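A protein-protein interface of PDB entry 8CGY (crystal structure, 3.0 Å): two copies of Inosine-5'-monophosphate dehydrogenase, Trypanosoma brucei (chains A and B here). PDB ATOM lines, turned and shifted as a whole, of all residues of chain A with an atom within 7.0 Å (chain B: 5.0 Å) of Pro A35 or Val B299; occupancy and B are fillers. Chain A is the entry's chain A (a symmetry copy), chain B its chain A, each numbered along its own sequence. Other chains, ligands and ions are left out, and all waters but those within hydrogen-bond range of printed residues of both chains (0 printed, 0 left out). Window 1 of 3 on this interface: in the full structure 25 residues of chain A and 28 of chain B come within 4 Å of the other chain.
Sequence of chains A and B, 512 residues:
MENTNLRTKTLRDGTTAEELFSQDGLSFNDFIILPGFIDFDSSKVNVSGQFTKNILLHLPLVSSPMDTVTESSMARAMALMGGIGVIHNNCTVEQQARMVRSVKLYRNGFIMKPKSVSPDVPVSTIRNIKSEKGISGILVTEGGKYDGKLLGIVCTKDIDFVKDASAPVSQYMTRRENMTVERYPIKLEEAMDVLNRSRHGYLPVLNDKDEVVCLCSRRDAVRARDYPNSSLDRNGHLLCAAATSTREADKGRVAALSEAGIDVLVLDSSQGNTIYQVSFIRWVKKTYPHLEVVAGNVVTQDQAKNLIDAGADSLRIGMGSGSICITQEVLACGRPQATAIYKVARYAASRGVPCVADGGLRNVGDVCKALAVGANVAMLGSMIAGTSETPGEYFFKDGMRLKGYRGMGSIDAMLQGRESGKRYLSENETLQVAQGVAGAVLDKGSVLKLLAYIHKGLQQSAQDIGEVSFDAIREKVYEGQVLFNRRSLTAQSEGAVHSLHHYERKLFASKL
Hydrophobic or aromatic side chains of chain A that line the printed part of chain B: Leu A34 and Pro A35.
Printed residues of chain B that touch a printed residue of chain A: Gln B271, Val B299, Thr B300, Gln B301, Gln B303, Met B319, Cys B333, Gly B334 and Arg B335.
Hydrophobic or aromatic side chains of chain B within 4 Å of the printed part of chain A: Val B299 and Met B319.
Among the printed residues, Asp or Glu carboxylates within 4 Å of a Lys or Arg side-chain nitrogen of the other chain: Asp A13 with Arg B335.
Lys A9 touches none of the printed residues of chain B.
Of the printed residues of chain B, Ile A33 touches Cys B333 and Gly B334.
Pro A35 touches just these residues of chain B: Gln B271, Val B299, Gln B303, Met B319 and Cys B333.
Printed residues of chain B within 4 Å of Asp A464: Gln B271 (3.0 Å), Met B319 (3.8 Å) and Cys B333 (3.6 Å).
Val B298 touches none of the printed residues of chain A.
Of the printed residues of chain A, Val B299 touches Pro A35.
Of the printed residues of chain A, Thr B300 touches Asp A13 (3.5 Å).
Of the printed residues of chain A, Gln B301 touches Asp A13.
The nearest printed residue of chain B that does not touch Phe A37 is Gln B303 (6.2 Å).
Among the printed residues, pairs that only touch across the chains: Asp A13 with Thr B300 (3.5 Å), Leu A34 with Gly B334 (3.3 Å), Leu A34 with Arg B335 (3.7 Å), Pro A35 with Gln B271 (3.0 Å), Pro A35 with Val B299 (3.4 Å), Pro A35 with Gln B303 (3.2 Å), Pro A35 with Met B319 (3.9 Å), Phe A37 with Gln B271 (3.97 Å), Asp A464 with Met B319 (3.8 Å) and Asp A464 with Cys B333 (3.6 Å).
The side-chain amide nitrogen (NE2) of Gln B271 sits at hydrogen-bond distance from the backbone carbonyl oxygen (O) of Gly A36 (2.5 Å).
The side-chain amide oxygen (OE1) of Gln B271 lies close to the backbone carbonyl oxygen (O) of Asp A464 (3.0 Å).
The side-chain carboxylate (OD2) of Asp A13 sits at hydrogen-bond distance from the backbone NH (N) of Gln B301, 2.9 Å away.
SG of Cys B333 sits close to O of Ile A33, at 3.6 Å.
O of Ile A33 lies within hydrogen-bond range of N of Gly B334, at 3.1 Å.
The side-chain carboxylate (OD1) of Asp A13 lies within salt-bridge range of the guanidinium group (NH2) of Arg B335 (2.9 Å).
NE of Arg B335 sits close to ND2 of Asn A485, 2.8 Å away.
N of Pro A35 sits close to SG of Cys B333, at 3.7 Å.
No position is printed for both chains.
Of the 18 pairs that touch across the chains among the printed residues, none has its exchanged pair printed and touching as well.
The guanidinium group (NH1) of Arg B335 sits at hydrogen-bond distance from the backbone carbonyl oxygen (O) of Val B299 (2.5 Å).
The backbone NH (N) of Thr B300 sits at hydrogen-bond distance from the side-chain amide oxygen (OE1) of Gln B303, at 3.1 Å.
N of Arg B335 is in hydrogen-bond range of O of Met B319 (3.5 Å).
The backbone carbonyl oxygen (O) of Leu A483 sits at hydrogen-bond distance from the backbone NH (N) of Leu A34.
The backbone NH of Gly A36 lies within hydrogen-bond range of the backbone carbonyl oxygen of Asp A464 (3.1 Å).
N of Gly A36 is in hydrogen-bond range of O of Ile A465.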
ATOM      1  N   LYS A   9      32.662 -12.926   2.874  1.00  0.00           N
ATOM      2  CA  LYS A   9      31.718 -13.845   2.254  1.00  0.00           C
ATOM      3  C   LYS A   9      32.060 -13.984   0.777  1.00  0.00           C
ATOM      4  O   LYS A   9      32.120 -12.982   0.055  1.00  0.00           O
ATOM      5  CB  LYS A   9      30.286 -13.339   2.432  1.00  0.00           C
ATOM      6  CG  LYS A   9      29.785 -13.372   3.870  1.00  0.00           C
ATOM      7  CD  LYS A   9      28.560 -12.487   4.125  1.00  0.00           C
ATOM      8  CE  LYS A   9      28.491 -12.173   5.625  1.00  0.00           C
ATOM      9  NZ  LYS A   9      27.596 -11.055   6.052  1.00  0.00           N
ATOM     10  N   ASP A  13      25.568 -16.094   0.341  1.00  0.00           N
ATOM     11  CA  ASP A  13      24.207 -16.599   0.549  1.00  0.00           C
ATOM     12  C   ASP A  13      23.381 -15.575   1.317  1.00  0.00           C
ATOM     13  O   ASP A  13      23.406 -15.545   2.551  1.00  0.00           O
ATOM     14  CB  ASP A  13      24.230 -17.941   1.297  1.00  0.00           C
ATOM     15  CG  ASP A  13      22.841 -18.396   1.761  1.00  0.00           C
ATOM     16  OD1 ASP A  13      21.828 -17.953   1.178  1.00  0.00           O
ATOM     17  OD2 ASP A  13      22.763 -19.198   2.720  1.00  0.00           O
ATOM     18  N   ILE A  33      18.451  -9.101   9.206  1.00  0.00           N
ATOM     19  CA  ILE A  33      19.870  -9.032   8.855  1.00  0.00           C
ATOM     20  C   ILE A  33      20.523 -10.376   9.146  1.00  0.00           C
ATOM     21  O   ILE A  33      20.369 -10.926  10.240  1.00  0.00           O
ATOM     22  CB  ILE A  33      20.580  -7.900   9.620  1.00  0.00           C
ATOM     23  CG1 ILE A  33      19.767  -6.605   9.563  1.00  0.00           C
ATOM     24  CG2 ILE A  33      21.970  -7.667   9.042  1.00  0.00           C
ATOM     25  CD1 ILE A  33      20.396  -5.464  10.340  1.00  0.00           C
ATOM     26  N   LEU A  34      21.261 -10.902   8.170  1.00  0.00           N
ATOM     27  CA  LEU A  34      21.854 -12.217   8.345  1.00  0.00           C
ATOM     28  C   LEU A  34      23.166 -12.132   9.120  1.00  0.00           C
ATOM     29  O   LEU A  34      23.919 -11.164   8.984  1.00  0.00           O
ATOM     30  CB  LEU A  34      22.102 -12.877   6.997  1.00  0.00           C
ATOM     31  CG  LEU A  34      20.861 -13.054   6.132  1.00  0.00           C
ATOM     32  CD1 LEU A  34      21.263 -13.539   4.758  1.00  0.00           C
ATOM     33  CD2 LEU A  34      19.904 -14.030   6.784  1.00  0.00           C
ATOM     34  N   PRO A  35      23.471 -13.151   9.915  1.00  0.00           N
ATOM     35  CA  PRO A  35      24.657 -13.097  10.775  1.00  0.00           C
ATOM     36  C   PRO A  35      25.955 -13.239   9.990  1.00  0.00           C
ATOM     37  O   PRO A  35      25.997 -13.789   8.885  1.00  0.00           O
ATOM     38  CB  PRO A  35      24.452 -14.278  11.726  1.00  0.00           C
ATOM     39  CG  PRO A  35      23.637 -15.246  10.927  1.00  0.00           C
ATOM     40  CD  PRO A  35      22.720 -14.408  10.078  1.00  0.00           C
ATOM     41  N   GLY A  36      27.031 -12.735  10.599  1.00  0.00           N
ATOM     42  CA  GLY A  36      28.352 -12.747   9.994  1.00  0.00           C
ATOM     43  C   GLY A  36      29.371 -13.583  10.746  1.00  0.00           C
ATOM     44  O   GLY A  36      29.112 -14.754  11.036  1.00  0.00           O
ATOM     45  N   PHE A  37      30.534 -13.008  11.063  1.00  0.00           N
ATOM     46  CA  PHE A  37      31.613 -13.731  11.732  1.00  0.00           C
ATOM     47  C   PHE A  37      32.136 -12.926  12.915  1.00  0.00           C
ATOM     48  O   PHE A  37      32.481 -11.748  12.766  1.00  0.00           O
ATOM     49  CB  PHE A  37      32.760 -14.040  10.763  1.00  0.00           C
ATOM     50  CG  PHE A  37      33.954 -14.681  11.421  1.00  0.00           C
ATOM     51  CD1 PHE A  37      34.031 -16.057  11.557  1.00  0.00           C
ATOM     52  CD2 PHE A  37      34.999 -13.906  11.902  1.00  0.00           C
ATOM     53  CE1 PHE A  37      35.129 -16.650  12.162  1.00  0.00           C
ATOM     54  CE2 PHE A  37      36.098 -14.491  12.508  1.00  0.00           C
ATOM     55  CZ  PHE A  37      36.162 -15.864  12.637  1.00  0.00           C
ATOM     56  N   GLN A 463      27.588  -7.275  17.035  1.00  0.00           N
ATOM     57  CA  GLN A 463      28.404  -8.476  17.186  1.00  0.00           C
ATOM     58  C   GLN A 463      27.843  -9.624  16.353  1.00  0.00           C
ATOM     59  O   GLN A 463      28.584 -10.300  15.630  1.00  0.00           O
ATOM     60  CB  GLN A 463      28.505  -8.879  18.655  1.00  0.00           C
ATOM     61  CG  GLN A 463      29.436 -10.060  18.882  1.00  0.00           C
ATOM     62  CD  GLN A 463      29.390 -10.572  20.304  1.00  0.00           C
ATOM     63  OE1 GLN A 463      28.315 -10.822  20.847  1.00  0.00           O
ATOM     64  NE2 GLN A 463      30.558 -10.725  20.915  1.00  0.00           N
ATOM     65  N   ASP A 464      26.529  -9.852  16.433  1.00  0.00           N
ATOM     66  CA  ASP A 464      25.927 -10.922  15.643  1.00  0.00           C
ATOM     67  C   ASP A 464      26.137 -10.685  14.150  1.00  0.00           C
ATOM     68  O   ASP A 464      26.509 -11.608  13.415  1.00  0.00           O
ATOM     69  CB  ASP A 464      24.435 -11.050  15.975  1.00  0.00           C
ATOM     70  CG  ASP A 464      24.170 -11.907  17.213  1.00  0.00           C
ATOM     71  OD1 ASP A 464      24.707 -13.033  17.298  1.00  0.00           O
ATOM     72  OD2 ASP A 464      23.414 -11.457  18.103  1.00  0.00           O
ATOM     73  N   ILE A 465      25.927  -9.448  13.690  1.00  0.00           N
ATOM     74  CA  ILE A 465      26.105  -9.120  12.276  1.00  0.00           C
ATOM     75  C   ILE A 465      27.547  -9.328  11.832  1.00  0.00           C
ATOM     76  O   ILE A 465      27.811  -9.570  10.648  1.00  0.00           O
ATOM     77  CB  ILE A 465      25.631  -7.675  12.010  1.00  0.00           C
ATOM     78  CG1 ILE A 465      24.124  -7.549  12.239  1.00  0.00           C
ATOM     79  CG2 ILE A 465      25.976  -7.230  10.599  1.00  0.00           C
ATOM     80  CD1 ILE A 465      23.605  -6.148  12.002  1.00  0.00           C
ATOM     81  N   GLY A 466      28.498  -9.231  12.756  1.00  0.00           N
ATOM     82  CA  GLY A 466      29.882  -9.568  12.475  1.00  0.00           C
ATOM     83  C   GLY A 466      30.825  -8.421  12.174  1.00  0.00           C
ATOM     84  O   GLY A 466      31.894  -8.665  11.601  1.00  0.00           O
ATOM     85  N   GLN A 481      28.650  -7.191   1.497  1.00  0.00           N
ATOM     86  CA  GLN A 481      29.228  -8.108   2.468  1.00  0.00           C
ATOM     87  C   GLN A 481      28.376  -8.264   3.717  1.00  0.00           C
ATOM     88  O   GLN A 481      28.572  -9.229   4.468  1.00  0.00           O
ATOM     89  CB  GLN A 481      30.635  -7.639   2.837  1.00  0.00           C
ATOM     90  CG  GLN A 481      31.654  -8.040   1.797  1.00  0.00           C
ATOM     91  CD  GLN A 481      31.758  -9.545   1.673  1.00  0.00           C
ATOM     92  OE1 GLN A 481      31.868 -10.251   2.673  1.00  0.00           O
ATOM     93  NE2 GLN A 481      31.709 -10.045   0.443  1.00  0.00           N
ATOM     94  N   LEU A 483      24.460  -8.927   4.426  1.00  0.00           N
ATOM     95  CA  LEU A 483      23.339  -9.386   3.626  1.00  0.00           C
ATOM     96  C   LEU A 483      22.091  -9.490   4.489  1.00  0.00           C
ATOM     97  O   LEU A 483      22.155  -9.637   5.712  1.00  0.00           O
ATOM     98  CB  LEU A 483      23.655 -10.731   2.963  1.00  0.00           C
ATOM     99  CG  LEU A 483      24.928 -10.668   2.123  1.00  0.00           C
ATOM    100  CD1 LEU A 483      25.297 -12.025   1.526  1.00  0.00           C
ATOM    101  CD2 LEU A 483      24.802  -9.605   1.034  1.00  0.00           C
ATOM    102  N   ASN A 485      17.592 -10.669   4.445  1.00  0.00           N
ATOM    103  CA  ASN A 485      16.647 -11.659   3.966  1.00  0.00           C
ATOM    104  C   ASN A 485      15.254 -11.110   4.197  1.00  0.00           C
ATOM    105  O   ASN A 485      14.871 -10.856   5.344  1.00  0.00           O
ATOM    106  CB  ASN A 485      16.852 -13.001   4.695  1.00  0.00           C
ATOM    107  CG  ASN A 485      16.599 -14.202   3.804  1.00  0.00           C
ATOM    108  OD1 ASN A 485      16.252 -14.069   2.632  1.00  0.00           O
ATOM    109  ND2 ASN A 485      16.783 -15.389   4.364  1.00  0.00           N
ATOM    110  N   GLN B 271      24.816 -17.922  17.647  1.00  0.00           N
ATOM    111  CA  GLN B 271      25.535 -17.934  16.379  1.00  0.00           C
ATOM    112  C   GLN B 271      26.889 -18.585  16.582  1.00  0.00           C
ATOM    113  O   GLN B 271      27.690 -18.113  17.396  1.00  0.00           O
ATOM    114  CB  GLN B 271      25.754 -16.545  15.811  1.00  0.00           C
ATOM    115  CG  GLN B 271      26.887 -16.613  14.818  1.00  0.00           C
ATOM    116  CD  GLN B 271      27.041 -15.345  14.068  1.00  0.00           C
ATOM    117  OE1 GLN B 271      26.182 -14.473  14.146  1.00  0.00           O
ATOM    118  NE2 GLN B 271      28.136 -15.214  13.334  1.00  0.00           N
ATOM    119  N   ASN B 297      24.906 -22.852  16.023  1.00  0.00           N
ATOM    120  CA  ASN B 297      23.720 -22.657  15.213  1.00  0.00           C
ATOM    121  C   ASN B 297      24.024 -21.738  14.045  1.00  0.00           C
ATOM    122  O   ASN B 297      24.737 -20.739  14.167  1.00  0.00           O
ATOM    123  CB  ASN B 297      22.554 -22.146  16.052  1.00  0.00           C
ATOM    124  CG  ASN B 297      21.802 -23.287  16.715  1.00  0.00           C
ATOM    125  OD1 ASN B 297      22.319 -23.924  17.636  1.00  0.00           O
ATOM    126  ND2 ASN B 297      20.595 -23.573  16.233  1.00  0.00           N
ATOM    127  N   VAL B 298      23.488 -22.114  12.883  1.00  0.00           N
ATOM    128  CA  VAL B 298      23.832 -21.476  11.624  1.00  0.00           C
ATOM    129  C   VAL B 298      22.544 -21.234  10.849  1.00  0.00           C
ATOM    130  O   VAL B 298      21.512 -21.854  11.102  1.00  0.00           O
ATOM    131  CB  VAL B 298      24.824 -22.333  10.819  1.00  0.00           C
ATOM    132  CG1 VAL B 298      25.106 -21.722   9.484  1.00  0.00           C
ATOM    133  CG2 VAL B 298      26.109 -22.493  11.625  1.00  0.00           C
ATOM    134  N   VAL B 299      22.586 -20.240   9.960  1.00  0.00           N
ATOM    135  CA  VAL B 299      21.458 -20.002   9.066  1.00  0.00           C
ATOM    136  C   VAL B 299      21.913 -19.723   7.637  1.00  0.00           C
ATOM    137  O   VAL B 299      21.086 -19.677   6.717  1.00  0.00           O
ATOM    138  CB  VAL B 299      20.560 -18.869   9.596  1.00  0.00           C
ATOM    139  CG1 VAL B 299      19.831 -19.330  10.847  1.00  0.00           C
ATOM    140  CG2 VAL B 299      21.379 -17.620   9.876  1.00  0.00           C
ATOM    141  N   THR B 300      23.215 -19.515   7.428  1.00  0.00           N
ATOM    142  CA  THR B 300      23.717 -19.163   6.106  1.00  0.00           C
ATOM    143  C   THR B 300      24.858 -20.076   5.686  1.00  0.00           C
ATOM    144  O   THR B 300      25.653 -20.537   6.511  1.00  0.00           O
ATOM    145  CB  THR B 300      24.208 -17.716   6.040  1.00  0.00           C
ATOM    146  OG1 THR B 300      25.495 -17.621   6.667  1.00  0.00           O
ATOM    147  CG2 THR B 300      23.227 -16.797   6.741  1.00  0.00           C
ATOM    148  N   GLN B 301      24.941 -20.303   4.372  1.00  0.00           N
ATOM    149  CA  GLN B 301      26.027 -21.102   3.818  1.00  0.00           C
ATOM    150  C   GLN B 301      27.388 -20.498   4.136  1.00  0.00           C
ATOM    151  O   GLN B 301      28.376 -21.231   4.259  1.00  0.00           O
ATOM    152  CB  GLN B 301      25.844 -21.245   2.308  1.00  0.00           C
ATOM    153  CG  GLN B 301      24.579 -21.981   1.906  1.00  0.00           C
ATOM    154  CD  GLN B 301      24.282 -21.861   0.427  1.00  0.00           C
ATOM    155  OE1 GLN B 301      24.864 -21.026  -0.266  1.00  0.00           O
ATOM    156  NE2 GLN B 301      23.374 -22.694  -0.067  1.00  0.00           N
ATOM    157  N   GLN B 303      28.292 -19.078   6.995  1.00  0.00           N
ATOM    158  CA  GLN B 303      28.612 -19.652   8.301  1.00  0.00           C
ATOM    159  C   GLN B 303      28.957 -21.129   8.180  1.00  0.00           C
ATOM    160  O   GLN B 303      29.922 -21.605   8.788  1.00  0.00           O
ATOM    161  CB  GLN B 303      27.432 -19.494   9.258  1.00  0.00           C
ATOM    162  CG  GLN B 303      27.208 -18.128   9.872  1.00  0.00           C
ATOM    163  CD  GLN B 303      25.808 -18.018  10.446  1.00  0.00           C
ATOM    164  OE1 GLN B 303      24.829 -18.316   9.760  1.00  0.00           O
ATOM    165  NE2 GLN B 303      25.705 -17.619  11.710  1.00  0.00           N
ATOM    166  N   GLY B 318      19.401 -22.995  12.699  1.00  0.00           N
ATOM    167  CA  GLY B 318      18.349 -22.213  13.317  1.00  0.00           C
ATOM    168  C   GLY B 318      18.835 -20.933  13.965  1.00  0.00           C
ATOM    169  O   GLY B 318      19.908 -20.896  14.574  1.00  0.00           O
ATOM    170  N   MET B 319      18.049 -19.870  13.821  1.00  0.00           N
ATOM    171  CA  MET B 319      18.278 -18.607  14.508  1.00  0.00           C
ATOM    172  C   MET B 319      17.017 -17.766  14.413  1.00  0.00           C
ATOM    173  O   MET B 319      16.489 -17.555  13.317  1.00  0.00           O
ATOM    174  CB  MET B 319      19.468 -17.855  13.918  1.00  0.00           C
ATOM    175  CG  MET B 319      20.040 -16.778  14.836  1.00  0.00           C
ATOM    176  SD  MET B 319      21.317 -15.767  14.057  1.00  0.00           S
ATOM    177  CE  MET B 319      22.035 -14.979  15.493  1.00  0.00           C
ATOM    178  N   CYS B 333      18.726  -9.884  13.838  1.00  0.00           N
ATOM    179  CA  CYS B 333      19.650 -10.835  13.237  1.00  0.00           C
ATOM    180  C   CYS B 333      19.055 -12.236  13.315  1.00  0.00           C
ATOM    181  O   CYS B 333      18.639 -12.675  14.390  1.00  0.00           O
ATOM    182  CB  CYS B 333      20.999 -10.760  13.957  1.00  0.00           C
ATOM    183  SG  CYS B 333      22.382 -11.529  13.112  1.00  0.00           S
ATOM    184  N   GLY B 334      19.013 -12.930  12.181  1.00  0.00           N
ATOM    185  CA  GLY B 334      18.395 -14.246  12.108  1.00  0.00           C
ATOM    186  C   GLY B 334      17.958 -14.552  10.680  1.00  0.00           C
ATOM    187  O   GLY B 334      18.404 -13.907   9.733  1.00  0.00           O
ATOM    188  N   ARG B 335      17.074 -15.562  10.550  1.00  0.00           N
ATOM    189  CA  ARG B 335      16.617 -15.976   9.220  1.00  0.00           C
ATOM    190  C   ARG B 335      15.458 -16.972   9.270  1.00  0.00           C
ATOM    191  O   ARG B 335      15.474 -17.893  10.096  1.00  0.00           O
ATOM    192  CB  ARG B 335      17.786 -16.578   8.443  1.00  0.00           C
ATOM    193  CG  ARG B 335      17.491 -16.840   6.985  1.00  0.00           C
ATOM    194  CD  ARG B 335      18.642 -17.571   6.330  1.00  0.00           C
ATOM    195  NE  ARG B 335      18.627 -17.400   4.883  1.00  0.00           N
ATOM    196  CZ  ARG B 335      19.538 -17.901   4.063  1.00  0.00           C
ATOM    197  NH1 ARG B 335      20.543 -18.636   4.513  1.00  0.00           N
ATOM    198  NH2 ARG B 335      19.443 -17.657   2.762  1.00  0.00           N
ATOM    199  N   GLN B 337      13.136 -20.114   9.043  1.00  0.00           N
ATOM    200  CA  GLN B 337      13.679 -21.458   9.229  1.00  0.00           C
ATOM    201  C   GLN B 337      13.684 -22.252   7.934  1.00  0.00           C
ATOM    202  O   GLN B 337      14.689 -22.882   7.589  1.00  0.00           O
ATOM    203  CB  GLN B 337      12.890 -22.212  10.297  1.00  0.00           C
ATOM    204  CG  GLN B 337      13.625 -22.347  11.613  1.00  0.00           C
ATOM    205  CD  GLN B 337      15.085 -22.724  11.438  1.00  0.00           C
ATOM    206  OE1 GLN B 337      15.938 -21.864  11.222  1.00  0.00           O
ATOM    207  NE2 GLN B 337      15.380 -24.014  11.541  1.00  0.00           N
ATOM    208  N   ALA B 340      16.399 -21.133   5.747  1.00  0.00           N
ATOM    209  CA  ALA B 340      17.694 -21.426   6.357  1.00  0.00           C
ATOM    210  C   ALA B 340      18.034 -22.907   6.254  1.00  0.00           C
ATOM    211  O   ALA B 340      19.174 -23.268   5.942  1.00  0.00           O
ATOM    212  CB  ALA B 340      17.716 -20.971   7.815  1.00  0.00           C
ATOM    213  N   VAL B 344      21.298 -24.073   3.937  1.00  0.00           N
ATOM    214  CA  VAL B 344      22.448 -24.636   4.630  1.00  0.00           C
ATOM    215  C   VAL B 344      22.545 -26.133   4.382  1.00  0.00           C
ATOM    216  O   VAL B 344      23.634 -26.664   4.137  1.00  0.00           O
ATOM    217  CB  VAL B 344      22.391 -24.319   6.132  1.00  0.00           C
ATOM    218  CG1 VAL B 344      23.472 -25.101   6.853  1.00  0.00           C
ATOM    219  CG2 VAL B 344      22.571 -22.829   6.355  1.00  0.00           C
